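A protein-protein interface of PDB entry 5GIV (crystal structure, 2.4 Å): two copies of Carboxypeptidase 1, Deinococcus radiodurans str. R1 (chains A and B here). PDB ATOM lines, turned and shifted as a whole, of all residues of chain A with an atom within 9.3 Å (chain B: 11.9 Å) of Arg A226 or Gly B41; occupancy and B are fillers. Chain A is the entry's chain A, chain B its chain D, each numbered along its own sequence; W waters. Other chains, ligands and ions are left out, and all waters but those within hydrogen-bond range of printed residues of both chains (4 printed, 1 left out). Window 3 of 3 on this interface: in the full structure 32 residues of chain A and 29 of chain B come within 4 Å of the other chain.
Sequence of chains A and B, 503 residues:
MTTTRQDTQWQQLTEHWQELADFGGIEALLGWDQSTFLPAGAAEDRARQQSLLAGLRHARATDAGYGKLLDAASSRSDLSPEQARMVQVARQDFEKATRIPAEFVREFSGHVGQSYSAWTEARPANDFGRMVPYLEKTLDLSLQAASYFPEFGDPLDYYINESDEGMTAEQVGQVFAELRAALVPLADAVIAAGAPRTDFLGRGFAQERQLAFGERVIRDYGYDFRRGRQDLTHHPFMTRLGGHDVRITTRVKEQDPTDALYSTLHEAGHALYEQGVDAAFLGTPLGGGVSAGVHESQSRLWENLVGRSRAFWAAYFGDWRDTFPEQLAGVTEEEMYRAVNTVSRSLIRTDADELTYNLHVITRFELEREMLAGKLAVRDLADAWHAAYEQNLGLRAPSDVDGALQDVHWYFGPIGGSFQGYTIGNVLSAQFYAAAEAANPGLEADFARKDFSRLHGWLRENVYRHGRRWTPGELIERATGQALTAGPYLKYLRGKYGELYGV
O of Arg A226 sits at hydrogen-bond distance from N of Gly B41, 2.7 Å away. The guanidinium group of Arg A247 lies within salt-bridge range of the side-chain carboxylate of Asp B33, 2.8 Å away.
The side-chain carboxylate of Asp A245 lies within salt-bridge range of the guanidinium group of Arg A247, at 2.7 Å. The side-chain hydroxyl of Tyr A223 sits at hydrogen-bond distance from the backbone NH of Arg A229. O of Asp B33 sits at hydrogen-bond distance from N of Leu B38 (2.9 Å). OD1 of Asp B45 is in salt-bridge range of NH1 of Arg B48 (2.7 Å). The side-chain carboxylate (OD1) of Asp A224 sits at hydrogen-bond distance from the backbone NH (N) of Arg A226 (2.9 Å). OD2 of Asp B33 lies within salt-bridge range of NH1 of Arg B46, at 2.8 Å.
Among the printed residues, merely in contact across the chains: Phe A225 with Pro B39 (3.9 Å), Arg A226 with Pro B39 (3.5 Å), Arg A226 with Ala B40 (3.6 Å), Gly A228 with Pro B39 (3.5 Å), Arg A229 with Phe B37 (3.2 Å), Gly A243 with Asp B45 (3.8 Å), His A244 with Gly B41 (3.3 Å), His A244 with Ala B42 (3.6 Å), His A244 with Asp B45 (3.3 Å), Asp A245 with Leu B38 (3.6 Å), Asp A245 with Pro B39 (3.3 Å), Arg A247 with Phe B37 (3.97 Å), Arg A247 with Leu B38 (3.6 Å) and Arg A247 with Pro B39 (3.5 Å).
No residue of chain B comes within 4 Å of Asp A224. Phe A225 touches one residue of chain B. Printed residues of chain B within 4 Å of Arg A226: Pro B39, Ala B40 and Gly B41. No residue of chain B comes within 4 Å of Arg A227. Gly A228 touches one residue of chain B. Of chain B, only Asp B45 comes within 4 Å of Gly A243. Of chain B, only Gly B41 (3.3 Å), Ala B42 (3.6 Å) and Asp B45 (3.3 Å) come within 4 Å of His A244. Printed residues of chain B within 4 Å of Asp A245: Leu B38 (3.6 Å) and Pro B39 (3.3 Å). Of the printed residues of chain A, Phe B37 touches Arg A229 (3.2 Å) and Arg A247 (3.97 Å). Ala B40 touches just one residue of chain A: Arg A226 (3.6 Å). Gly B41 touches just these residues of chain A: Arg A226 and His A244. Ala B42 touches just one residue of chain A: His A244. The nearest residue of chain B that does not touch Arg A226 is Ala B42 (4.3 Å).
Printed residues of chain B that touch a printed residue of chain A: Asp B33, Phe B37, Leu B38, Pro B39, Ala B40, Gly B41, Ala B42 and Asp B45. Hydrophobic or aromatic side chains of chain B within 4 Å of the printed part of chain A: Phe B37, Leu B38, Pro B39 and Ala B42. Of the 17 printed residues of chain A, 8 touch a printed residue of chain B. Hydrophobic or aromatic side chains of chain A that line the printed part of chain B: His A244. Among the printed residues, 16 pairs touch across the chains.
No position is printed for both chains.
Water W3 bridges the backbone carbonyl oxygen (O) of Phe B37 (2.7 Å) and the guanidinium group (NH1) of Arg A229 (2.8 Å). Water W1 bridges OD2 of Asp A245 (2.7 Å) and NH2 of Arg B46 (2.9 Å). Water W2 lies within hydrogen-bond range of the backbone NH (N) of His A244 (2.7 Å) and the side-chain carboxylate (OD2) of Asp B45 (2.8 Å). Water W4 lies within hydrogen-bond range of N of Gly A243 (2.9 Å), NH2 of Arg B48 (3.0 Å) and OD1 of Asp B45 (3.1 Å).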
ATOM      1  N   ARG A 219     -31.350  -1.602 -20.000  1.00  0.00           N
ATOM      2  CA  ARG A 219     -30.734  -1.144 -21.236  1.00  0.00           C
ATOM      3  C   ARG A 219     -31.461   0.085 -21.771  1.00  0.00           C
ATOM      4  O   ARG A 219     -30.828   1.085 -22.120  1.00  0.00           O
ATOM      5  CB  ARG A 219     -30.723  -2.274 -22.263  1.00  0.00           C
ATOM      6  CG  ARG A 219     -30.050  -1.924 -23.565  1.00  0.00           C
ATOM      7  CD  ARG A 219     -31.051  -1.869 -24.699  1.00  0.00           C
ATOM      8  NE  ARG A 219     -31.403  -3.197 -25.210  1.00  0.00           N
ATOM      9  CZ  ARG A 219     -32.641  -3.677 -25.246  1.00  0.00           C
ATOM     10  NH1 ARG A 219     -33.645  -2.940 -24.803  1.00  0.00           N
ATOM     11  NH2 ARG A 219     -32.875  -4.883 -25.741  1.00  0.00           N
ATOM     12  N   GLY A 222     -30.768   3.219 -19.856  1.00  0.00           N
ATOM     13  CA  GLY A 222     -29.522   3.872 -20.202  1.00  0.00           C
ATOM     14  C   GLY A 222     -28.300   3.186 -19.632  1.00  0.00           C
ATOM     15  O   GLY A 222     -27.186   3.722 -19.724  1.00  0.00           O
ATOM     16  N   TYR A 223     -28.485   2.021 -19.009  1.00  0.00           N
ATOM     17  CA  TYR A 223     -27.345   1.271 -18.495  1.00  0.00           C
ATOM     18  C   TYR A 223     -26.489   0.801 -19.661  1.00  0.00           C
ATOM     19  O   TYR A 223     -27.009   0.277 -20.650  1.00  0.00           O
ATOM     20  CB  TYR A 223     -27.804   0.081 -17.658  1.00  0.00           C
ATOM     21  CG  TYR A 223     -26.675  -0.680 -16.999  1.00  0.00           C
ATOM     22  CD1 TYR A 223     -25.979  -0.132 -15.937  1.00  0.00           C
ATOM     23  CD2 TYR A 223     -26.318  -1.959 -17.429  1.00  0.00           C
ATOM     24  CE1 TYR A 223     -24.949  -0.823 -15.331  1.00  0.00           C
ATOM     25  CE2 TYR A 223     -25.293  -2.657 -16.825  1.00  0.00           C
ATOM     26  CZ  TYR A 223     -24.612  -2.085 -15.776  1.00  0.00           C
ATOM     27  OH  TYR A 223     -23.593  -2.767 -15.170  1.00  0.00           O
ATOM     28  N   ASP A 224     -25.180   1.017 -19.559  1.00  0.00           N
ATOM     29  CA  ASP A 224     -24.248   0.782 -20.658  1.00  0.00           C
ATOM     30  C   ASP A 224     -23.535  -0.543 -20.418  1.00  0.00           C
ATOM     31  O   ASP A 224     -22.605  -0.624 -19.610  1.00  0.00           O
ATOM     32  CB  ASP A 224     -23.256   1.934 -20.752  1.00  0.00           C
ATOM     33  CG  ASP A 224     -22.372   1.851 -21.981  1.00  0.00           C
ATOM     34  OD1 ASP A 224     -22.441   0.839 -22.719  1.00  0.00           O
ATOM     35  OD2 ASP A 224     -21.596   2.805 -22.200  1.00  0.00           O
ATOM     36  N   PHE A 225     -23.934  -1.576 -21.152  1.00  0.00           N
ATOM     37  CA  PHE A 225     -23.284  -2.867 -20.964  1.00  0.00           C
ATOM     38  C   PHE A 225     -21.874  -2.904 -21.532  1.00  0.00           C
ATOM     39  O   PHE A 225     -21.126  -3.844 -21.237  1.00  0.00           O
ATOM     40  CB  PHE A 225     -24.124  -3.976 -21.593  1.00  0.00           C
ATOM     41  CG  PHE A 225     -25.307  -4.381 -20.759  1.00  0.00           C
ATOM     42  CD1 PHE A 225     -25.170  -5.318 -19.741  1.00  0.00           C
ATOM     43  CD2 PHE A 225     -26.558  -3.829 -20.991  1.00  0.00           C
ATOM     44  CE1 PHE A 225     -26.259  -5.696 -18.970  1.00  0.00           C
ATOM     45  CE2 PHE A 225     -27.651  -4.202 -20.226  1.00  0.00           C
ATOM     46  CZ  PHE A 225     -27.500  -5.133 -19.212  1.00  0.00           C
ATOM     47  N   ARG A 226     -21.464  -1.892 -22.287  1.00  0.00           N
ATOM     48  CA  ARG A 226     -20.056  -1.832 -22.638  1.00  0.00           C
ATOM     49  C   ARG A 226     -19.206  -1.345 -21.466  1.00  0.00           C
ATOM     50  O   ARG A 226     -17.973  -1.401 -21.540  1.00  0.00           O
ATOM     51  CB  ARG A 226     -19.886  -0.978 -23.901  1.00  0.00           C
ATOM     52  CG  ARG A 226     -20.666  -1.609 -25.079  1.00  0.00           C
ATOM     53  CD  ARG A 226     -20.472  -0.908 -26.428  1.00  0.00           C
ATOM     54  NE  ARG A 226     -19.286  -1.389 -27.133  1.00  0.00           N
ATOM     55  CZ  ARG A 226     -18.093  -0.828 -27.018  1.00  0.00           C
ATOM     56  NH1 ARG A 226     -17.065  -1.314 -27.698  1.00  0.00           N
ATOM     57  NH2 ARG A 226     -17.928   0.188 -26.184  1.00  0.00           N
ATOM     58  N   ARG A 227     -19.841  -0.876 -20.391  1.00  0.00           N
ATOM     59  CA  ARG A 227     -19.155  -0.415 -19.192  1.00  0.00           C
ATOM     60  C   ARG A 227     -19.733  -1.069 -17.944  1.00  0.00           C
ATOM     61  O   ARG A 227     -19.764  -0.465 -16.873  1.00  0.00           O
ATOM     62  CB  ARG A 227     -19.166   1.113 -19.077  1.00  0.00           C
ATOM     63  CG  ARG A 227     -18.637   1.784 -20.331  1.00  0.00           C
ATOM     64  CD  ARG A 227     -18.482   3.293 -20.217  1.00  0.00           C
ATOM     65  NE  ARG A 227     -19.705   4.011 -19.880  1.00  0.00           N
ATOM     66  CZ  ARG A 227     -19.804   4.856 -18.859  1.00  0.00           C
ATOM     67  NH1 ARG A 227     -18.748   5.083 -18.074  1.00  0.00           N
ATOM     68  NH2 ARG A 227     -20.950   5.479 -18.634  1.00  0.00           N
ATOM     69  N   GLY A 228     -20.190  -2.305 -18.067  1.00  0.00           N
ATOM     70  CA  GLY A 228     -20.743  -3.004 -16.927  1.00  0.00           C
ATOM     71  C   GLY A 228     -21.314  -4.339 -17.342  1.00  0.00           C
ATOM     72  O   GLY A 228     -21.220  -4.758 -18.500  1.00  0.00           O
ATOM     73  N   ARG A 229     -21.917  -5.002 -16.364  1.00  0.00           N
ATOM     74  CA  ARG A 229     -22.576  -6.283 -16.576  1.00  0.00           C
ATOM     75  C   ARG A 229     -23.357  -6.609 -15.312  1.00  0.00           C
ATOM     76  O   ARG A 229     -23.203  -5.952 -14.280  1.00  0.00           O
ATOM     77  CB  ARG A 229     -21.568  -7.396 -16.909  1.00  0.00           C
ATOM     78  CG  ARG A 229     -20.485  -7.588 -15.866  1.00  0.00           C
ATOM     79  CD  ARG A 229     -19.658  -8.860 -16.119  1.00  0.00           C
ATOM     80  NE  ARG A 229     -20.439 -10.086 -15.933  1.00  0.00           N
ATOM     81  CZ  ARG A 229     -20.931 -10.813 -16.926  1.00  0.00           C
ATOM     82  NH1 ARG A 229     -20.729 -10.458 -18.190  1.00  0.00           N
ATOM     83  NH2 ARG A 229     -21.638 -11.897 -16.656  1.00  0.00           N
ATOM     84  N   GLY A 242     -13.828  -0.232 -11.970  1.00  0.00           N
ATOM     85  CA  GLY A 242     -12.972   0.660 -12.739  1.00  0.00           C
ATOM     86  C   GLY A 242     -13.775   1.820 -13.307  1.00  0.00           C
ATOM     87  O   GLY A 242     -15.011   1.865 -13.225  1.00  0.00           O
ATOM     88  N   GLY A 243     -13.046   2.746 -13.935  1.00  0.00           N
ATOM     89  CA  GLY A 243     -13.681   3.914 -14.523  1.00  0.00           C
ATOM     90  C   GLY A 243     -14.746   3.592 -15.552  1.00  0.00           C
ATOM     91  O   GLY A 243     -15.625   4.421 -15.792  1.00  0.00           O
ATOM     92  N   HIS A 244     -14.673   2.427 -16.189  1.00  0.00           N
ATOM     93  CA  HIS A 244     -15.638   2.017 -17.204  1.00  0.00           C
ATOM     94  C   HIS A 244     -16.160   0.618 -16.917  1.00  0.00           C
ATOM     95  O   HIS A 244     -16.477  -0.147 -17.833  1.00  0.00           O
ATOM     96  CB  HIS A 244     -15.023   2.095 -18.597  1.00  0.00           C
ATOM     97  CG  HIS A 244     -14.584   3.475 -18.972  1.00  0.00           C
ATOM     98  ND1 HIS A 244     -15.464   4.435 -19.425  1.00  0.00           N
ATOM     99  CD2 HIS A 244     -13.364   4.061 -18.956  1.00  0.00           C
ATOM    100  CE1 HIS A 244     -14.806   5.554 -19.667  1.00  0.00           C
ATOM    101  NE2 HIS A 244     -13.531   5.356 -19.391  1.00  0.00           N
ATOM    102  N   ASP A 245     -16.320   0.293 -15.630  1.00  0.00           N
ATOM    103  CA  ASP A 245     -16.676  -1.057 -15.195  1.00  0.00           C
ATOM    104  C   ASP A 245     -17.543  -0.917 -13.938  1.00  0.00           C
ATOM    105  O   ASP A 245     -17.036  -0.924 -12.813  1.00  0.00           O
ATOM    106  CB  ASP A 245     -15.423  -1.876 -14.925  1.00  0.00           C
ATOM    107  CG  ASP A 245     -15.679  -3.369 -14.905  1.00  0.00           C
ATOM    108  OD1 ASP A 245     -16.841  -3.796 -15.011  1.00  0.00           O
ATOM    109  OD2 ASP A 245     -14.699  -4.120 -14.785  1.00  0.00           O
ATOM    110  N   VAL A 246     -18.849  -0.756 -14.143  1.00  0.00           N
ATOM    111  CA  VAL A 246     -19.800  -0.596 -13.047  1.00  0.00           C
ATOM    112  C   VAL A 246     -20.749  -1.785 -13.094  1.00  0.00           C
ATOM    113  O   VAL A 246     -21.648  -1.842 -13.939  1.00  0.00           O
ATOM    114  CB  VAL A 246     -20.553   0.732 -13.125  1.00  0.00           C
ATOM    115  CG1 VAL A 246     -21.448   0.878 -11.920  1.00  0.00           C
ATOM    116  CG2 VAL A 246     -19.546   1.874 -13.171  1.00  0.00           C
ATOM    117  N   ARG A 247     -20.543  -2.744 -12.197  1.00  0.00           N
ATOM    118  CA  ARG A 247     -21.249  -4.016 -12.256  1.00  0.00           C
ATOM    119  C   ARG A 247     -22.377  -4.080 -11.234  1.00  0.00           C
ATOM    120  O   ARG A 247     -22.299  -3.500 -10.147  1.00  0.00           O
ATOM    121  CB  ARG A 247     -20.272  -5.169 -12.043  1.00  0.00           C
ATOM    122  CG  ARG A 247     -19.065  -5.068 -12.962  1.00  0.00           C
ATOM    123  CD  ARG A 247     -18.307  -6.382 -13.066  1.00  0.00           C
ATOM    124  NE  ARG A 247     -17.125  -6.236 -13.910  1.00  0.00           N
ATOM    125  CZ  ARG A 247     -16.198  -7.175 -14.088  1.00  0.00           C
ATOM    126  NH1 ARG A 247     -16.300  -8.354 -13.485  1.00  0.00           N
ATOM    127  NH2 ARG A 247     -15.165  -6.930 -14.875  1.00  0.00           N
ATOM    128  N   GLN A 275     -22.132   5.514 -13.699  1.00  0.00           N
ATOM    129  CA  GLN A 275     -21.801   5.560 -15.120  1.00  0.00           C
ATOM    130  C   GLN A 275     -21.953   6.953 -15.707  1.00  0.00           C
ATOM    131  O   GLN A 275     -21.435   7.210 -16.796  1.00  0.00           O
ATOM    132  CB  GLN A 275     -22.660   4.565 -15.912  1.00  0.00           C
ATOM    133  CG  GLN A 275     -22.205   3.097 -15.780  1.00  0.00           C
ATOM    134  CD  GLN A 275     -22.901   2.166 -16.763  1.00  0.00           C
ATOM    135  OE1 GLN A 275     -23.989   2.468 -17.278  1.00  0.00           O
ATOM    136  NE2 GLN A 275     -22.277   1.026 -17.029  1.00  0.00           N
ATOM    137  N   LEU A 282     -13.093  10.802 -13.399  1.00  0.00           N
ATOM    138  CA  LEU A 282     -12.731   9.413 -13.161  1.00  0.00           C
ATOM    139  C   LEU A 282     -11.252   9.316 -12.826  1.00  0.00           C
ATOM    140  O   LEU A 282     -10.417   9.992 -13.429  1.00  0.00           O
ATOM    141  CB  LEU A 282     -13.056   8.549 -14.382  1.00  0.00           C
ATOM    142  CG  LEU A 282     -14.505   8.573 -14.902  1.00  0.00           C
ATOM    143  CD1 LEU A 282     -14.658   7.632 -16.108  1.00  0.00           C
ATOM    144  CD2 LEU A 282     -15.509   8.241 -13.790  1.00  0.00           C
ATOM    145  N   ASP B  33     -10.509 -12.460 -14.972  1.00  0.00           N
ATOM    146  CA  ASP B  33     -11.683 -11.633 -15.206  1.00  0.00           C
ATOM    147  C   ASP B  33     -11.589 -10.926 -16.550  1.00  0.00           C
ATOM    148  O   ASP B  33     -12.604 -10.764 -17.241  1.00  0.00           O
ATOM    149  CB  ASP B  33     -11.841 -10.621 -14.067  1.00  0.00           C
ATOM    150  CG  ASP B  33     -13.005  -9.685 -14.279  1.00  0.00           C
ATOM    151  OD1 ASP B  33     -14.158 -10.110 -14.052  1.00  0.00           O
ATOM    152  OD2 ASP B  33     -12.762  -8.526 -14.670  1.00  0.00           O
ATOM    153  N   GLN B  34     -10.378 -10.540 -16.955  1.00  0.00           N
ATOM    154  CA  GLN B  34     -10.209  -9.886 -18.245  1.00  0.00           C
ATOM    155  C   GLN B  34     -10.645 -10.785 -19.398  1.00  0.00           C
ATOM    156  O   GLN B  34     -11.224 -10.303 -20.379  1.00  0.00           O
ATOM    157  CB  GLN B  34      -8.761  -9.453 -18.442  1.00  0.00           C
ATOM    158  CG  GLN B  34      -8.552  -8.828 -19.796  1.00  0.00           C
ATOM    159  CD  GLN B  34      -7.119  -8.793 -20.187  1.00  0.00           C
ATOM    160  OE1 GLN B  34      -6.577  -9.803 -20.646  1.00  0.00           O
ATOM    161  NE2 GLN B  34      -6.472  -7.641 -20.006  1.00  0.00           N
ATOM    162  N   THR B  36     -12.856 -13.364 -19.225  1.00  0.00           N
ATOM    163  CA  THR B  36     -14.190 -13.930 -19.087  1.00  0.00           C
ATOM    164  C   THR B  36     -15.277 -12.863 -19.047  1.00  0.00           C
ATOM    165  O   THR B  36     -16.201 -12.894 -19.866  1.00  0.00           O
ATOM    166  CB  THR B  36     -14.247 -14.816 -17.837  1.00  0.00           C
ATOM    167  OG1 THR B  36     -13.769 -14.078 -16.709  1.00  0.00           O
ATOM    168  CG2 THR B  36     -13.379 -16.038 -18.009  1.00  0.00           C
ATOM    169  N   PHE B  37     -15.182 -11.893 -18.132  1.00  0.00           N
ATOM    170  CA  PHE B  37     -16.312 -11.023 -17.833  1.00  0.00           C
ATOM    171  C   PHE B  37     -16.041  -9.531 -17.981  1.00  0.00           C
ATOM    172  O   PHE B  37     -16.992  -8.746 -17.901  1.00  0.00           O
ATOM    173  CB  PHE B  37     -16.818 -11.300 -16.406  1.00  0.00           C
ATOM    174  CG  PHE B  37     -17.248 -12.721 -16.189  1.00  0.00           C
ATOM    175  CD1 PHE B  37     -18.359 -13.230 -16.850  1.00  0.00           C
ATOM    176  CD2 PHE B  37     -16.555 -13.551 -15.314  1.00  0.00           C
ATOM    177  CE1 PHE B  37     -18.763 -14.541 -16.652  1.00  0.00           C
ATOM    178  CE2 PHE B  37     -16.954 -14.860 -15.113  1.00  0.00           C
ATOM    179  CZ  PHE B  37     -18.061 -15.354 -15.784  1.00  0.00           C
ATOM    180  N   LEU B  38     -14.803  -9.117 -18.219  1.00  0.00           N
ATOM    181  CA  LEU B  38     -14.498  -7.694 -18.356  1.00  0.00           C
ATOM    182  C   LEU B  38     -15.342  -7.074 -19.465  1.00  0.00           C
ATOM    183  O   LEU B  38     -15.377  -7.610 -20.582  1.00  0.00           O
ATOM    184  CB  LEU B  38     -13.013  -7.493 -18.655  1.00  0.00           C
ATOM    185  CG  LEU B  38     -12.465  -6.060 -18.706  1.00  0.00           C
ATOM    186  CD1 LEU B  38     -12.526  -5.406 -17.340  1.00  0.00           C
ATOM    187  CD2 LEU B  38     -11.042  -6.075 -19.234  1.00  0.00           C
ATOM    188  N   PRO B  39     -16.072  -5.993 -19.193  1.00  0.00           N
ATOM    189  CA  PRO B  39     -16.846  -5.331 -20.256  1.00  0.00           C
ATOM    190  C   PRO B  39     -15.939  -4.709 -21.313  1.00  0.00           C
ATOM    191  O   PRO B  39     -14.806  -4.304 -21.044  1.00  0.00           O
ATOM    192  CB  PRO B  39     -17.644  -4.257 -19.502  1.00  0.00           C
ATOM    193  CG  PRO B  39     -17.690  -4.738 -18.069  1.00  0.00           C
ATOM    194  CD  PRO B  39     -16.372  -5.445 -17.857  1.00  0.00           C
ATOM    195  N   ALA B  40     -16.489  -4.559 -22.521  1.00  0.00           N
ATOM    196  CA  ALA B  40     -15.660  -4.186 -23.667  1.00  0.00           C
ATOM    197  C   ALA B  40     -14.974  -2.836 -23.468  1.00  0.00           C
ATOM    198  O   ALA B  40     -13.804  -2.669 -23.830  1.00  0.00           O
ATOM    199  CB  ALA B  40     -16.503  -4.179 -24.940  1.00  0.00           C
ATOM    200  N   GLY B  41     -15.663  -1.869 -22.871  1.00  0.00           N
ATOM    201  CA  GLY B  41     -15.051  -0.566 -22.735  1.00  0.00           C
ATOM    202  C   GLY B  41     -14.094  -0.407 -21.582  1.00  0.00           C
ATOM    203  O   GLY B  41     -13.658   0.713 -21.302  1.00  0.00           O
ATOM    204  N   ALA B  42     -13.735  -1.488 -20.894  1.00  0.00           N
ATOM    205  CA  ALA B  42     -12.917  -1.392 -19.696  1.00  0.00           C
ATOM    206  C   ALA B  42     -11.502  -1.922 -19.899  1.00  0.00           C
ATOM    207  O   ALA B  42     -10.769  -2.091 -18.919  1.00  0.00           O
ATOM    208  CB  ALA B  42     -13.593  -2.130 -18.537  1.00  0.00           C
ATOM    209  N   ALA B  43     -11.087  -2.147 -21.148  1.00  0.00           N
ATOM    210  CA  ALA B  43      -9.806  -2.804 -21.406  1.00  0.00           C
ATOM    211  C   ALA B  43      -8.631  -1.973 -20.906  1.00  0.00           C
ATOM    212  O   ALA B  43      -7.695  -2.506 -20.292  1.00  0.00           O
ATOM    213  CB  ALA B  43      -9.657  -3.077 -22.903  1.00  0.00           C
ATOM    214  N   GLU B  44      -8.661  -0.665 -21.147  1.00  0.00           N
ATOM    215  CA  GLU B  44      -7.488   0.157 -20.875  1.00  0.00           C
ATOM    216  C   GLU B  44      -7.224   0.255 -19.378  1.00  0.00           C
ATOM    217  O   GLU B  44      -6.081   0.116 -18.931  1.00  0.00           O
ATOM    218  CB  GLU B  44      -7.673   1.542 -21.495  1.00  0.00           C
ATOM    219  CG  GLU B  44      -6.436   2.413 -21.472  1.00  0.00           C
ATOM    220  CD  GLU B  44      -6.675   3.778 -22.100  1.00  0.00           C
ATOM    221  OE1 GLU B  44      -7.031   4.732 -21.367  1.00  0.00           O
ATOM    222  OE2 GLU B  44      -6.514   3.892 -23.336  1.00  0.00           O
ATOM    223  N   ASP B  45      -8.272   0.487 -18.589  1.00  0.00           N
ATOM    224  CA  ASP B  45      -8.105   0.598 -17.146  1.00  0.00           C
ATOM    225  C   ASP B  45      -7.620  -0.717 -16.545  1.00  0.00           C
ATOM    226  O   ASP B  45      -6.796  -0.721 -15.622  1.00  0.00           O
ATOM    227  CB  ASP B  45      -9.426   1.018 -16.507  1.00  0.00           C
ATOM    228  CG  ASP B  45      -9.817   2.431 -16.856  1.00  0.00           C
ATOM    229  OD1 ASP B  45      -8.948   3.327 -16.843  1.00  0.00           O
ATOM    230  OD2 ASP B  45     -11.009   2.647 -17.149  1.00  0.00           O
ATOM    231  N   ARG B  46      -8.133  -1.847 -17.042  1.00  0.00           N
ATOM    232  CA  ARG B  46      -7.702  -3.132 -16.508  1.00  0.00           C
ATOM    233  C   ARG B  46      -6.213  -3.351 -16.747  1.00  0.00           C
ATOM    234  O   ARG B  46      -5.490  -3.805 -15.847  1.00  0.00           O
ATOM    235  CB  ARG B  46      -8.533  -4.259 -17.115  1.00  0.00           C
ATOM    236  CG  ARG B  46      -8.031  -5.649 -16.759  1.00  0.00           C
ATOM    237  CD  ARG B  46      -7.946  -5.862 -15.247  1.00  0.00           C
ATOM    238  NE  ARG B  46      -9.194  -5.538 -14.559  1.00  0.00           N
ATOM    239  CZ  ARG B  46     -10.210  -6.381 -14.431  1.00  0.00           C
ATOM    240  NH1 ARG B  46     -10.127  -7.600 -14.937  1.00  0.00           N
ATOM    241  NH2 ARG B  46     -11.308  -6.008 -13.794  1.00  0.00           N
ATOM    242  N   ALA B  47      -5.724  -2.975 -17.938  1.00  0.00           N
ATOM    243  CA  ALA B  47      -4.301  -3.116 -18.230  1.00  0.00           C
ATOM    244  C   ALA B  47      -3.472  -2.253 -17.295  1.00  0.00           C
ATOM    245  O   ALA B  47      -2.387  -2.658 -16.852  1.00  0.00           O
ATOM    246  CB  ALA B  47      -4.020  -2.751 -19.687  1.00  0.00           C
ATOM    247  N   ARG B  48      -3.977  -1.061 -16.964  1.00  0.00           N
ATOM    248  CA  ARG B  48      -3.254  -0.208 -16.033  1.00  0.00           C
ATOM    249  C   ARG B  48      -3.258  -0.821 -14.636  1.00  0.00           C
ATOM    250  O   ARG B  48      -2.235  -0.799 -13.940  1.00  0.00           O
ATOM    251  CB  ARG B  48      -3.876   1.187 -16.013  1.00  0.00           C
ATOM    252  CG  ARG B  48      -3.030   2.230 -15.320  1.00  0.00           C
ATOM    253  CD  ARG B  48      -3.683   3.600 -15.321  1.00  0.00           C
ATOM    254  NE  ARG B  48      -4.973   3.575 -14.641  1.00  0.00           N
ATOM    255  CZ  ARG B  48      -6.156   3.582 -15.253  1.00  0.00           C
ATOM    256  NH1 ARG B  48      -6.236   3.644 -16.578  1.00  0.00           N
ATOM    257  NH2 ARG B  48      -7.266   3.541 -14.532  1.00  0.00           N
ATOM    258  N   GLN B  49      -4.397  -1.380 -14.215  1.00  0.00           N
ATOM    259  CA  GLN B  49      -4.444  -2.110 -12.952  1.00  0.00           C
ATOM    260  C   GLN B  49      -3.424  -3.240 -12.931  1.00  0.00           C
ATOM    261  O   GLN B  49      -2.732  -3.445 -11.924  1.00  0.00           O
ATOM    262  CB  GLN B  49      -5.850  -2.657 -12.703  1.00  0.00           C
ATOM    263  CG  GLN B  49      -6.884  -1.595 -12.427  1.00  0.00           C
ATOM    264  CD  GLN B  49      -8.283  -2.150 -12.476  1.00  0.00           C
ATOM    265  OE1 GLN B  49      -8.496  -3.296 -12.885  1.00  0.00           O
ATOM    266  NE2 GLN B  49      -9.253  -1.343 -12.056  1.00  0.00           N
ATOM    267  N   GLU B 121      -6.005  -6.297 -34.608  1.00  0.00           N
ATOM    268  CA  GLU B 121      -6.554  -5.660 -35.795  1.00  0.00           C
ATOM    269  C   GLU B 121      -5.897  -6.124 -37.085  1.00  0.00           C
ATOM    270  O   GLU B 121      -6.590  -6.313 -38.092  1.00  0.00           O
ATOM    271  CB  GLU B 121      -6.405  -4.142 -35.685  1.00  0.00           C
ATOM    272  CG  GLU B 121      -6.868  -3.564 -34.354  1.00  0.00           C
ATOM    273  CD  GLU B 121      -6.674  -2.065 -34.283  1.00  0.00           C
ATOM    274  OE1 GLU B 121      -6.000  -1.496 -35.176  1.00  0.00           O
ATOM    275  OE2 GLU B 121      -7.180  -1.457 -33.318  1.00  0.00           O
HETATM  276  O   HOH W   1     -12.267  -3.278 -13.958  1.00  0.00           O
HETATM  277  O   HOH W   2     -12.818   0.511 -16.625  1.00  0.00           O
HETATM  278  O   HOH W   3     -19.137  -8.552 -19.452  1.00  0.00           O
HETATM  279  O   HOH W   4     -10.188   2.854 -14.031  1.00  0.00           O
